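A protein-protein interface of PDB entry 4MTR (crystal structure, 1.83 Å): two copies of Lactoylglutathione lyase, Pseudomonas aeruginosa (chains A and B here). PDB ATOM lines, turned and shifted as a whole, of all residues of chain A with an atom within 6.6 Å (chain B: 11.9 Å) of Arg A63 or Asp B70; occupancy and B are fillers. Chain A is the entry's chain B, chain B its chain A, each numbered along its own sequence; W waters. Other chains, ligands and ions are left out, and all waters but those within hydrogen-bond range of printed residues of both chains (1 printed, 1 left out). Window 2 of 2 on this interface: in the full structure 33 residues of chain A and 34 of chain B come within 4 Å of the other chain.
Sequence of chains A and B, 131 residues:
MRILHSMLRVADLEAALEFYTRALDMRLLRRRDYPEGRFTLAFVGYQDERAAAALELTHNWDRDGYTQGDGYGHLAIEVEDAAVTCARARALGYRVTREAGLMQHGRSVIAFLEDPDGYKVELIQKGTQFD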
ATOM      1  N   ARG A   9       7.003  -7.644 -20.562  1.00  0.00           N
ATOM      2  CA  ARG A   9       6.766  -7.475 -19.117  1.00  0.00           C
ATOM      3  C   ARG A   9       5.773  -6.318 -18.898  1.00  0.00           C
ATOM      4  O   ARG A   9       5.874  -5.265 -19.524  1.00  0.00           O
ATOM      5  CB  ARG A   9       8.061  -7.245 -18.362  1.00  0.00           C
ATOM      6  CG  ARG A   9       9.037  -8.397 -18.528  1.00  0.00           C
ATOM      7  CD  ARG A   9      10.154  -8.292 -17.497  1.00  0.00           C
ATOM      8  NE  ARG A   9      11.124  -9.371 -17.671  1.00  0.00           N
ATOM      9  CZ  ARG A   9      12.105  -9.365 -18.570  1.00  0.00           C
ATOM     10  NH1 ARG A   9      12.288  -8.311 -19.357  1.00  0.00           N
ATOM     11  NH2 ARG A   9      12.904 -10.410 -18.691  1.00  0.00           N
ATOM     12  N   VAL A  10       4.763  -6.568 -18.089  1.00  0.00           N
ATOM     13  CA  VAL A  10       3.632  -5.647 -17.864  1.00  0.00           C
ATOM     14  C   VAL A  10       3.519  -5.296 -16.375  1.00  0.00           C
ATOM     15  O   VAL A  10       3.713  -6.176 -15.531  1.00  0.00           O
ATOM     16  CB  VAL A  10       2.300  -6.236 -18.425  1.00  0.00           C
ATOM     17  CG1 VAL A  10       2.351  -6.422 -19.951  1.00  0.00           C
ATOM     18  CG2 VAL A  10       1.921  -7.539 -17.743  1.00  0.00           C
ATOM     19  N   ALA A  11       3.202  -4.025 -16.068  1.00  0.00           N
ATOM     20  CA  ALA A  11       3.061  -3.525 -14.696  1.00  0.00           C
ATOM     21  C   ALA A  11       1.869  -4.143 -13.992  1.00  0.00           C
ATOM     22  O   ALA A  11       1.928  -4.420 -12.797  1.00  0.00           O
ATOM     23  CB  ALA A  11       2.906  -2.005 -14.721  1.00  0.00           C
ATOM     24  N   HIS A  59       4.401 -10.674 -15.341  1.00  0.00           N
ATOM     25  CA  HIS A  59       4.443  -9.654 -14.298  1.00  0.00           C
ATOM     26  C   HIS A  59       5.340 -10.153 -13.141  1.00  0.00           C
ATOM     27  O   HIS A  59       5.152 -11.271 -12.676  1.00  0.00           O
ATOM     28  CB  HIS A  59       3.053  -9.190 -13.799  1.00  0.00           C
ATOM     29  CG  HIS A  59       3.185  -8.164 -12.697  1.00  0.00           C
ATOM     30  ND1 HIS A  59       2.759  -8.441 -11.394  1.00  0.00           N
ATOM     31  CD2 HIS A  59       3.841  -6.977 -12.694  1.00  0.00           C
ATOM     32  CE1 HIS A  59       3.108  -7.393 -10.672  1.00  0.00           C
ATOM     33  NE2 HIS A  59       3.771  -6.488 -11.400  1.00  0.00           N
ATOM     34  N   ASN A  60       6.379  -9.385 -12.771  1.00  0.00           N
ATOM     35  CA  ASN A  60       7.262  -9.709 -11.654  1.00  0.00           C
ATOM     36  C   ASN A  60       6.617  -9.043 -10.411  1.00  0.00           C
ATOM     37  O   ASN A  60       6.392  -7.832 -10.407  1.00  0.00           O
ATOM     38  CB  ASN A  60       8.672  -9.140 -11.883  1.00  0.00           C
ATOM     39  CG  ASN A  60       9.348  -9.716 -13.082  1.00  0.00           C
ATOM     40  OD1 ASN A  60       9.838 -10.849 -13.059  1.00  0.00           O
ATOM     41  ND2 ASN A  60       9.345  -8.958 -14.167  1.00  0.00           N
ATOM     42  N   TRP A  61       6.253  -9.847  -9.403  1.00  0.00           N
ATOM     43  CA  TRP A  61       5.538  -9.376  -8.201  1.00  0.00           C
ATOM     44  C   TRP A  61       6.179  -8.159  -7.523  1.00  0.00           C
ATOM     45  O   TRP A  61       5.465  -7.248  -7.112  1.00  0.00           O
ATOM     46  CB  TRP A  61       5.311 -10.553  -7.218  1.00  0.00           C
ATOM     47  CG  TRP A  61       4.553 -11.724  -7.791  1.00  0.00           C
ATOM     48  CD1 TRP A  61       4.025 -11.842  -9.045  1.00  0.00           C
ATOM     49  CD2 TRP A  61       4.311 -12.978  -7.136  1.00  0.00           C
ATOM     50  NE1 TRP A  61       3.453 -13.086  -9.206  1.00  0.00           N
ATOM     51  CE2 TRP A  61       3.611 -13.801  -8.048  1.00  0.00           C
ATOM     52  CE3 TRP A  61       4.581 -13.470  -5.843  1.00  0.00           C
ATOM     53  CZ2 TRP A  61       3.192 -15.096  -7.718  1.00  0.00           C
ATOM     54  CZ3 TRP A  61       4.157 -14.749  -5.516  1.00  0.00           C
ATOM     55  CH2 TRP A  61       3.486 -15.554  -6.450  1.00  0.00           C
ATOM     56  N   ASP A  62       7.518  -8.101  -7.492  1.00  0.00           N
ATOM     57  CA  ASP A  62       8.287  -7.021  -6.869  1.00  0.00           C
ATOM     58  C   ASP A  62       8.489  -5.748  -7.742  1.00  0.00           C
ATOM     59  O   ASP A  62       9.260  -4.866  -7.341  1.00  0.00           O
ATOM     60  CB  ASP A  62       9.655  -7.563  -6.371  1.00  0.00           C
ATOM     61  CG  ASP A  62       9.588  -8.789  -5.455  1.00  0.00           C
ATOM     62  OD1 ASP A  62      10.480  -9.670  -5.571  1.00  0.00           O
ATOM     63  OD2 ASP A  62       8.621  -8.888  -4.651  1.00  0.00           O
ATOM     64  N   ARG A  63       7.802  -5.652  -8.910  1.00  0.00           N
ATOM     65  CA  ARG A  63       7.911  -4.500  -9.837  1.00  0.00           C
ATOM     66  C   ARG A  63       6.577  -3.761  -9.981  1.00  0.00           C
ATOM     67  O   ARG A  63       5.528  -4.404  -9.975  1.00  0.00           O
ATOM     68  CB  ARG A  63       8.391  -4.951 -11.244  1.00  0.00           C
ATOM     69  CG  ARG A  63       9.808  -5.554 -11.319  1.00  0.00           C
ATOM     70  CD  ARG A  63      10.965  -4.596 -11.050  1.00  0.00           C
ATOM     71  NE  ARG A  63      11.021  -3.468 -11.986  1.00  0.00           N
ATOM     72  CZ  ARG A  63      11.771  -3.444 -13.085  1.00  0.00           C
ATOM     73  NH1 ARG A  63      12.518  -4.493 -13.412  1.00  0.00           N
ATOM     74  NH2 ARG A  63      11.776  -2.377 -13.868  1.00  0.00           N
ATOM     75  N   ASP A  64       6.624  -2.429 -10.172  1.00  0.00           N
ATOM     76  CA  ASP A  64       5.439  -1.570 -10.372  1.00  0.00           C
ATOM     77  C   ASP A  64       5.325  -0.995 -11.806  1.00  0.00           C
ATOM     78  O   ASP A  64       4.306  -0.389 -12.161  1.00  0.00           O
ATOM     79  CB  ASP A  64       5.452  -0.401  -9.364  1.00  0.00           C
ATOM     80  CG  ASP A  64       5.373  -0.836  -7.906  1.00  0.00           C
ATOM     81  OD1 ASP A  64       4.366  -1.487  -7.529  1.00  0.00           O
ATOM     82  OD2 ASP A  64       6.318  -0.525  -7.140  1.00  0.00           O
ATOM     83  N   GLY A  65       6.385  -1.139 -12.577  1.00  0.00           N
ATOM     84  CA  GLY A  65       6.505  -0.622 -13.932  1.00  0.00           C
ATOM     85  C   GLY A  65       7.861  -0.986 -14.487  1.00  0.00           C
ATOM     86  O   GLY A  65       8.765  -1.355 -13.739  1.00  0.00           O
ATOM     87  N   TYR A  66       8.013  -0.896 -15.799  1.00  0.00           N
ATOM     88  CA  TYR A  66       9.258  -1.268 -16.474  1.00  0.00           C
ATOM     89  C   TYR A  66       9.865  -0.134 -17.260  1.00  0.00           C
ATOM     90  O   TYR A  66       9.151   0.773 -17.681  1.00  0.00           O
ATOM     91  CB  TYR A  66       9.014  -2.487 -17.386  1.00  0.00           C
ATOM     92  CG  TYR A  66       8.665  -3.714 -16.572  1.00  0.00           C
ATOM     93  CD1 TYR A  66       7.346  -3.992 -16.230  1.00  0.00           C
ATOM     94  CD2 TYR A  66       9.662  -4.526 -16.041  1.00  0.00           C
ATOM     95  CE1 TYR A  66       7.024  -5.069 -15.407  1.00  0.00           C
ATOM     96  CE2 TYR A  66       9.352  -5.593 -15.197  1.00  0.00           C
ATOM     97  CZ  TYR A  66       8.031  -5.870 -14.901  1.00  0.00           C
ATOM     98  OH  TYR A  66       7.697  -6.971 -14.151  1.00  0.00           O
ATOM     99  N   THR A  67      11.186  -0.192 -17.460  1.00  0.00           N
ATOM    100  CA  THR A  67      11.894   0.821 -18.232  1.00  0.00           C
ATOM    101  C   THR A  67      11.640   0.512 -19.687  1.00  0.00           C
ATOM    102  O   THR A  67      11.958  -0.579 -20.160  1.00  0.00           O
ATOM    103  CB  THR A  67      13.393   0.880 -17.874  1.00  0.00           C
ATOM    104  OG1 THR A  67      13.533   1.063 -16.466  1.00  0.00           O
ATOM    105  CG2 THR A  67      14.118   2.020 -18.581  1.00  0.00           C
ATOM    106  N   GLN A  68      11.012   1.435 -20.376  1.00  0.00           N
ATOM    107  CA  GLN A  68      10.753   1.224 -21.771  1.00  0.00           C
ATOM    108  C   GLN A  68      11.783   1.960 -22.617  1.00  0.00           C
ATOM    109  O   GLN A  68      11.977   3.168 -22.464  1.00  0.00           O
ATOM    110  CB  GLN A  68       9.300   1.588 -22.118  1.00  0.00           C
ATOM    111  CG  GLN A  68       8.778   0.937 -23.405  1.00  0.00           C
ATOM    112  CD  GLN A  68       9.210  -0.502 -23.601  1.00  0.00           C
ATOM    113  OE1 GLN A  68       9.072  -1.353 -22.710  1.00  0.00           O
ATOM    114  NE2 GLN A  68       9.760  -0.797 -24.769  1.00  0.00           N
ATOM    115  N   GLY A  69      12.486   1.205 -23.444  1.00  0.00           N
ATOM    116  CA  GLY A  69      13.505   1.758 -24.322  1.00  0.00           C
ATOM    117  C   GLY A  69      12.932   2.094 -25.678  1.00  0.00           C
ATOM    118  O   GLY A  69      11.716   2.211 -25.835  1.00  0.00           O
ATOM    119  N   TYR A 119       3.019  -0.259 -24.871  1.00  0.00           N
ATOM    120  CA  TYR A 119       3.549  -1.053 -26.001  1.00  0.00           C
ATOM    121  C   TYR A 119       2.697  -0.820 -27.225  1.00  0.00           C
ATOM    122  O   TYR A 119       1.471  -0.808 -27.091  1.00  0.00           O
ATOM    123  CB  TYR A 119       3.541  -2.543 -25.673  1.00  0.00           C
ATOM    124  CG  TYR A 119       4.486  -2.897 -24.561  1.00  0.00           C
ATOM    125  CD1 TYR A 119       5.861  -2.737 -24.714  1.00  0.00           C
ATOM    126  CD2 TYR A 119       4.024  -3.500 -23.396  1.00  0.00           C
ATOM    127  CE1 TYR A 119       6.750  -3.179 -23.737  1.00  0.00           C
ATOM    128  CE2 TYR A 119       4.901  -3.873 -22.376  1.00  0.00           C
ATOM    129  CZ  TYR A 119       6.260  -3.689 -22.545  1.00  0.00           C
ATOM    130  OH  TYR A 119       7.134  -4.077 -21.567  1.00  0.00           O
ATOM    131  N   LEU B   8      11.687  -5.062 -34.134  1.00  0.00           N
ATOM    132  CA  LEU B   8      12.860  -4.685 -33.320  1.00  0.00           C
ATOM    133  C   LEU B   8      13.750  -3.769 -34.119  1.00  0.00           C
ATOM    134  O   LEU B   8      13.949  -3.992 -35.310  1.00  0.00           O
ATOM    135  CB  LEU B   8      13.653  -5.946 -32.931  1.00  0.00           C
ATOM    136  CG  LEU B   8      12.907  -7.024 -32.091  1.00  0.00           C
ATOM    137  CD1 LEU B   8      13.799  -8.273 -31.859  1.00  0.00           C
ATOM    138  CD2 LEU B   8      12.422  -6.467 -30.749  1.00  0.00           C
ATOM    139  N   TYR B  66      20.410   1.596 -29.831  1.00  0.00           N
ATOM    140  CA  TYR B  66      19.148   1.927 -29.180  1.00  0.00           C
ATOM    141  C   TYR B  66      19.155   1.535 -27.723  1.00  0.00           C
ATOM    142  O   TYR B  66      19.902   0.635 -27.331  1.00  0.00           O
ATOM    143  CB  TYR B  66      17.995   1.166 -29.888  1.00  0.00           C
ATOM    144  CG  TYR B  66      17.837   1.535 -31.342  1.00  0.00           C
ATOM    145  CD1 TYR B  66      18.501   0.821 -32.341  1.00  0.00           C
ATOM    146  CD2 TYR B  66      16.995   2.571 -31.729  1.00  0.00           C
ATOM    147  CE1 TYR B  66      18.384   1.174 -33.681  1.00  0.00           C
ATOM    148  CE2 TYR B  66      16.848   2.918 -33.075  1.00  0.00           C
ATOM    149  CZ  TYR B  66      17.534   2.207 -34.047  1.00  0.00           C
ATOM    150  OH  TYR B  66      17.365   2.514 -35.381  1.00  0.00           O
ATOM    151  N   THR B  67      18.265   2.172 -26.944  1.00  0.00           N
ATOM    152  CA  THR B  67      18.050   1.904 -25.518  1.00  0.00           C
ATOM    153  C   THR B  67      17.093   0.708 -25.453  1.00  0.00           C
ATOM    154  O   THR B  67      16.010   0.766 -26.029  1.00  0.00           O
ATOM    155  CB  THR B  67      17.451   3.146 -24.839  1.00  0.00           C
ATOM    156  OG1 THR B  67      18.233   4.286 -25.179  1.00  0.00           O
ATOM    157  CG2 THR B  67      17.375   3.007 -23.320  1.00  0.00           C
ATOM    158  N   GLN B  68      17.481  -0.366 -24.779  1.00  0.00           N
ATOM    159  CA  GLN B  68      16.627  -1.547 -24.722  1.00  0.00           C
ATOM    160  C   GLN B  68      15.516  -1.559 -23.671  1.00  0.00           C
ATOM    161  O   GLN B  68      14.420  -2.036 -23.958  1.00  0.00           O
ATOM    162  CB  GLN B  68      17.467  -2.810 -24.651  1.00  0.00           C
ATOM    163  CG  GLN B  68      17.217  -3.715 -25.837  1.00  0.00           C
ATOM    164  CD  GLN B  68      18.300  -4.746 -25.966  1.00  0.00           C
ATOM    165  OE1 GLN B  68      18.335  -5.749 -25.235  1.00  0.00           O
ATOM    166  NE2 GLN B  68      19.213  -4.502 -26.895  1.00  0.00           N
ATOM    167  N   GLY B  69      15.806  -1.082 -22.467  1.00  0.00           N
ATOM    168  CA  GLY B  69      14.848  -1.087 -21.365  1.00  0.00           C
ATOM    169  C   GLY B  69      14.692  -2.492 -20.805  1.00  0.00           C
ATOM    170  O   GLY B  69      15.403  -3.408 -21.230  1.00  0.00           O
ATOM    171  N   ASP B  70      13.765  -2.701 -19.869  1.00  0.00           N
ATOM    172  CA  ASP B  70      13.593  -4.054 -19.345  1.00  0.00           C
ATOM    173  C   ASP B  70      12.176  -4.533 -19.515  1.00  0.00           C
ATOM    174  O   ASP B  70      11.783  -5.488 -18.861  1.00  0.00           O
ATOM    175  CB  ASP B  70      14.072  -4.166 -17.878  1.00  0.00           C
ATOM    176  CG  ASP B  70      13.382  -3.236 -16.902  1.00  0.00           C
ATOM    177  OD1 ASP B  70      13.763  -3.240 -15.709  1.00  0.00           O
ATOM    178  OD2 ASP B  70      12.446  -2.520 -17.322  1.00  0.00           O
ATOM    179  N   GLY B  71      11.403  -3.835 -20.349  1.00  0.00           N
ATOM    180  CA  GLY B  71      10.023  -4.214 -20.635  1.00  0.00           C
ATOM    181  C   GLY B  71       9.992  -5.356 -21.644  1.00  0.00           C
ATOM    182  O   GLY B  71       9.341  -6.387 -21.420  1.00  0.00           O
ATOM    183  N   TYR B  72      10.691  -5.177 -22.772  1.00  0.00           N
ATOM    184  CA  TYR B  72      10.775  -6.220 -23.786  1.00  0.00           C
ATOM    185  C   TYR B  72      11.473  -7.461 -23.240  1.00  0.00           C
ATOM    186  O   TYR B  72      12.542  -7.352 -22.648  1.00  0.00           O
ATOM    187  CB  TYR B  72      11.454  -5.732 -25.052  1.00  0.00           C
ATOM    188  CG  TYR B  72      11.588  -6.839 -26.073  1.00  0.00           C
ATOM    189  CD1 TYR B  72      10.469  -7.364 -26.706  1.00  0.00           C
ATOM    190  CD2 TYR B  72      12.820  -7.438 -26.324  1.00  0.00           C
ATOM    191  CE1 TYR B  72      10.580  -8.378 -27.643  1.00  0.00           C
ATOM    192  CE2 TYR B  72      12.943  -8.475 -27.250  1.00  0.00           C
ATOM    193  CZ  TYR B  72      11.816  -8.937 -27.907  1.00  0.00           C
ATOM    194  OH  TYR B  72      11.887  -9.974 -28.790  1.00  0.00           O
ATOM    195  N   GLY B  73      10.848  -8.617 -23.425  1.00  0.00           N
ATOM    196  CA  GLY B  73      11.368  -9.879 -22.914  1.00  0.00           C
ATOM    197  C   GLY B  73      12.280 -10.593 -23.887  1.00  0.00           C
ATOM    198  O   GLY B  73      13.507 -10.502 -23.782  1.00  0.00           O
ATOM    199  N   HIS B  74      11.684 -11.325 -24.837  1.00  0.00           N
ATOM    200  CA  HIS B  74      12.436 -12.147 -25.783  1.00  0.00           C
ATOM    201  C   HIS B  74      11.520 -12.598 -26.920  1.00  0.00           C
ATOM    202  O   HIS B  74      10.309 -12.325 -26.896  1.00  0.00           O
ATOM    203  CB  HIS B  74      12.988 -13.398 -25.032  1.00  0.00           C
ATOM    204  CG  HIS B  74      11.950 -14.226 -24.325  1.00  0.00           C
ATOM    205  ND1 HIS B  74      11.775 -14.147 -22.953  1.00  0.00           N
ATOM    206  CD2 HIS B  74      11.098 -15.158 -24.813  1.00  0.00           C
ATOM    207  CE1 HIS B  74      10.797 -14.984 -22.658  1.00  0.00           C
ATOM    208  NE2 HIS B  74      10.365 -15.628 -23.739  1.00  0.00           N
ATOM    209  N   GLU B 114      21.653 -14.435 -27.718  1.00  0.00           N
ATOM    210  CA  GLU B 114      21.558 -12.983 -27.824  1.00  0.00           C
ATOM    211  C   GLU B 114      21.942 -12.617 -29.263  1.00  0.00           C
ATOM    212  O   GLU B 114      22.978 -13.078 -29.787  1.00  0.00           O
ATOM    213  CB  GLU B 114      22.499 -12.264 -26.855  1.00  0.00           C
ATOM    214  CG  GLU B 114      22.066 -12.364 -25.411  1.00  0.00           C
ATOM    215  CD  GLU B 114      22.747 -11.344 -24.525  1.00  0.00           C
ATOM    216  OE1 GLU B 114      23.758 -10.754 -24.971  1.00  0.00           O
ATOM    217  OE2 GLU B 114      22.248 -11.103 -23.402  1.00  0.00           O
ATOM    218  N   ASP B 117      22.388  -7.053 -31.260  1.00  0.00           N
ATOM    219  CA  ASP B 117      21.920  -5.904 -30.513  1.00  0.00           C
ATOM    220  C   ASP B 117      21.611  -6.223 -29.037  1.00  0.00           C
ATOM    221  O   ASP B 117      21.206  -5.323 -28.305  1.00  0.00           O
ATOM    222  CB  ASP B 117      20.682  -5.287 -31.179  1.00  0.00           C
ATOM    223  CG  ASP B 117      20.994  -4.696 -32.523  1.00  0.00           C
ATOM    224  OD1 ASP B 117      21.210  -3.474 -32.591  1.00  0.00           O
ATOM    225  OD2 ASP B 117      20.986  -5.450 -33.507  1.00  0.00           O
ATOM    226  N   GLY B 118      21.763  -7.482 -28.641  1.00  0.00           N
ATOM    227  CA  GLY B 118      21.469  -7.938 -27.285  1.00  0.00           C
ATOM    228  C   GLY B 118      20.034  -8.395 -27.060  1.00  0.00           C
ATOM    229  O   GLY B 118      19.657  -8.693 -25.929  1.00  0.00           O
ATOM    230  N   TYR B 119      19.228  -8.529 -28.132  1.00  0.00           N
ATOM    231  CA  TYR B 119      17.860  -9.018 -27.962  1.00  0.00           C
ATOM    232  C   TYR B 119      17.937 -10.503 -27.715  1.00  0.00           C
ATOM    233  O   TYR B 119      18.661 -11.215 -28.410  1.00  0.00           O
ATOM    234  CB  TYR B 119      17.000  -8.776 -29.181  1.00  0.00           C
ATOM    235  CG  TYR B 119      16.765  -7.308 -29.468  1.00  0.00           C
ATOM    236  CD1 TYR B 119      16.010  -6.518 -28.600  1.00  0.00           C
ATOM    237  CD2 TYR B 119      17.250  -6.723 -30.630  1.00  0.00           C
ATOM    238  CE1 TYR B 119      15.733  -5.184 -28.896  1.00  0.00           C
ATOM    239  CE2 TYR B 119      16.991  -5.396 -30.927  1.00  0.00           C
ATOM    240  CZ  TYR B 119      16.245  -4.624 -30.055  1.00  0.00           C
ATOM    241  OH  TYR B 119      15.971  -3.329 -30.391  1.00  0.00           O
ATOM    242  N   LYS B 120      17.184 -10.964 -26.733  1.00  0.00           N
ATOM    243  CA  LYS B 120      17.217 -12.367 -26.360  1.00  0.00           C
ATOM    244  C   LYS B 120      16.310 -13.260 -27.219  1.00  0.00           C
ATOM    245  O   LYS B 120      15.148 -12.938 -27.501  1.00  0.00           O
ATOM    246  CB  LYS B 120      16.858 -12.523 -24.874  1.00  0.00           C
ATOM    247  CG  LYS B 120      17.847 -11.833 -23.934  1.00  0.00           C
ATOM    248  CD  LYS B 120      17.367 -11.886 -22.486  1.00  0.00           C
ATOM    249  CE  LYS B 120      18.394 -11.331 -21.531  1.00  0.00           C
ATOM    250  NZ  LYS B 120      19.618 -12.181 -21.471  1.00  0.00           N
HETATM  251  O   HOH W   1      14.467  -9.507 -21.231  1.00  0.00           O
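O of Asp B70 is in hydrogen-bond range of NH1 of Arg A9, at 2.9 Å.
The side-chain carboxylate of Asp B70 is in salt-bridge range of the guanidinium group of Arg A63, at 2.8 Å.
The backbone NH (N) of Thr A67 lies within hydrogen-bond range of the side-chain carboxylate (OD2) of Asp B70 (2.7 Å).
O of Gly B71 is in hydrogen-bond range of N of Arg A9.
O of Thr A67 is in hydrogen-bond range of N of Gly B71 (3.3 Å).
O of Gly B71 sits close to OH of Tyr A119.
NH1 of Arg A9 is in hydrogen-bond range of O of Tyr B72, 3.4 Å away.
The side-chain amide nitrogen (NE2) of Gln B68 is in hydrogen-bond range of the backbone carbonyl oxygen (O) of Asp B117 (2.6 Å).
O of Gly B118 sits close to OE1 of Gln B68 (3.3 Å).
OH of Tyr B72 sits close to O of His B74, 3.4 Å away.
The backbone carbonyl oxygen (O) of Arg A9 sits at hydrogen-bond distance from the side-chain hydroxyl (OH) of Tyr A119.
The side-chain hydroxyl of Tyr A66 lies within hydrogen-bond range of the side-chain amide nitrogen of Asn A60, 2.6 Å away.
NH2 of Arg A63 lies within hydrogen-bond range of O of Gly A65, at 3.2 Å.
Among the printed residues, pairs that only touch across the chains: Thr A67 with Gly B69 (3.2 Å), Gly A69 with Thr B67 (3.2 Å), Tyr A66 with Asp B70 (3.4 Å), Gln A68 with Gly B71 (3.7 Å), Gly A69 with Gln B68 (3.8 Å), Tyr A66 with Gly B71 (3.8 Å), Gly A69 with Gly B69 (3.9 Å), Tyr A119 with Tyr B72 (3.9 Å) and Arg A9 with Gly B73 (3.99 Å).
Of chain B, only Asp B70 (2.8 Å) comes within 4 Å of Arg A63.
No residue of chain B comes within 4 Å of Ala A11.
No residue of chain B comes within 4 Å of Asn A60.
No residue of chain B comes within 4 Å of Asp A64.
Gly A65 touches none of the printed residues of chain B.
Of chain B, only Asp B70 and Gly B71 come within 4 Å of Tyr A66.
Thr A67 touches just these residues of chain B: Gly B69 (3.2 Å), Asp B70 (2.7 Å) and Gly B71 (3.3 Å).
Printed residues of chain A within 4 Å of Gly B69: Thr A67 (3.2 Å) and Gly A69 (3.9 Å).
Printed residues of chain B within 4 Å of Gly A69: Thr B67, Gln B68 and Gly B69.
Printed residues of chain B within 4 Å of Arg A9: Asp B70 (2.9 Å), Gly B71 (2.8 Å), Tyr B72 (3.4 Å) and Gly B73 (3.99 Å).
Gly B118 touches none of the printed residues of chain A.
Tyr B119 touches none of the printed residues of chain A.
The nearest residue of chain B that does not touch Arg A63 is Gly B71 (6.7 Å).
The nearest residue of chain A that does not touch Asp B70 is Gln A68 (5.0 Å).
Of the 15 printed residues of chain B, 7 touch a printed residue of chain A.
Printed residues of chain A that touch a printed residue of chain B: Arg A9, Arg A63, Tyr A66, Thr A67, Gln A68, Gly A69 and Tyr A119.
Hydrophobic or aromatic side chains of chain A within 4 Å of the printed part of chain B: Tyr A66 and Tyr A119.
Among the printed residues, Asp or Glu carboxylates within 4 Å of a Lys or Arg side-chain nitrogen of the other chain: Arg A63 with Asp B70 (2.8 Å).
Thr A67 touches Gly B69, and with the chains exchanged Gly A69 touches Thr B67.
Gly A69 touches Gln B68, but with the chains exchanged Gln A68 does not touch Gly B69 (4.5 Å).
Gly B69 touches its own counterpart, Gly A69.
5 positions are printed for both chains.
Of the 16 pairs that touch across the chains among the printed residues, 3 have their exchanged pair printed and touching as well.
Water W1 lies within hydrogen-bond range of the backbone carbonyl oxygen of Gly B73 (2.9 Å), the guanidinium group of Arg A9 (3.1 Å) and the backbone carbonyl oxygen of Tyr B72 (3.2 Å).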
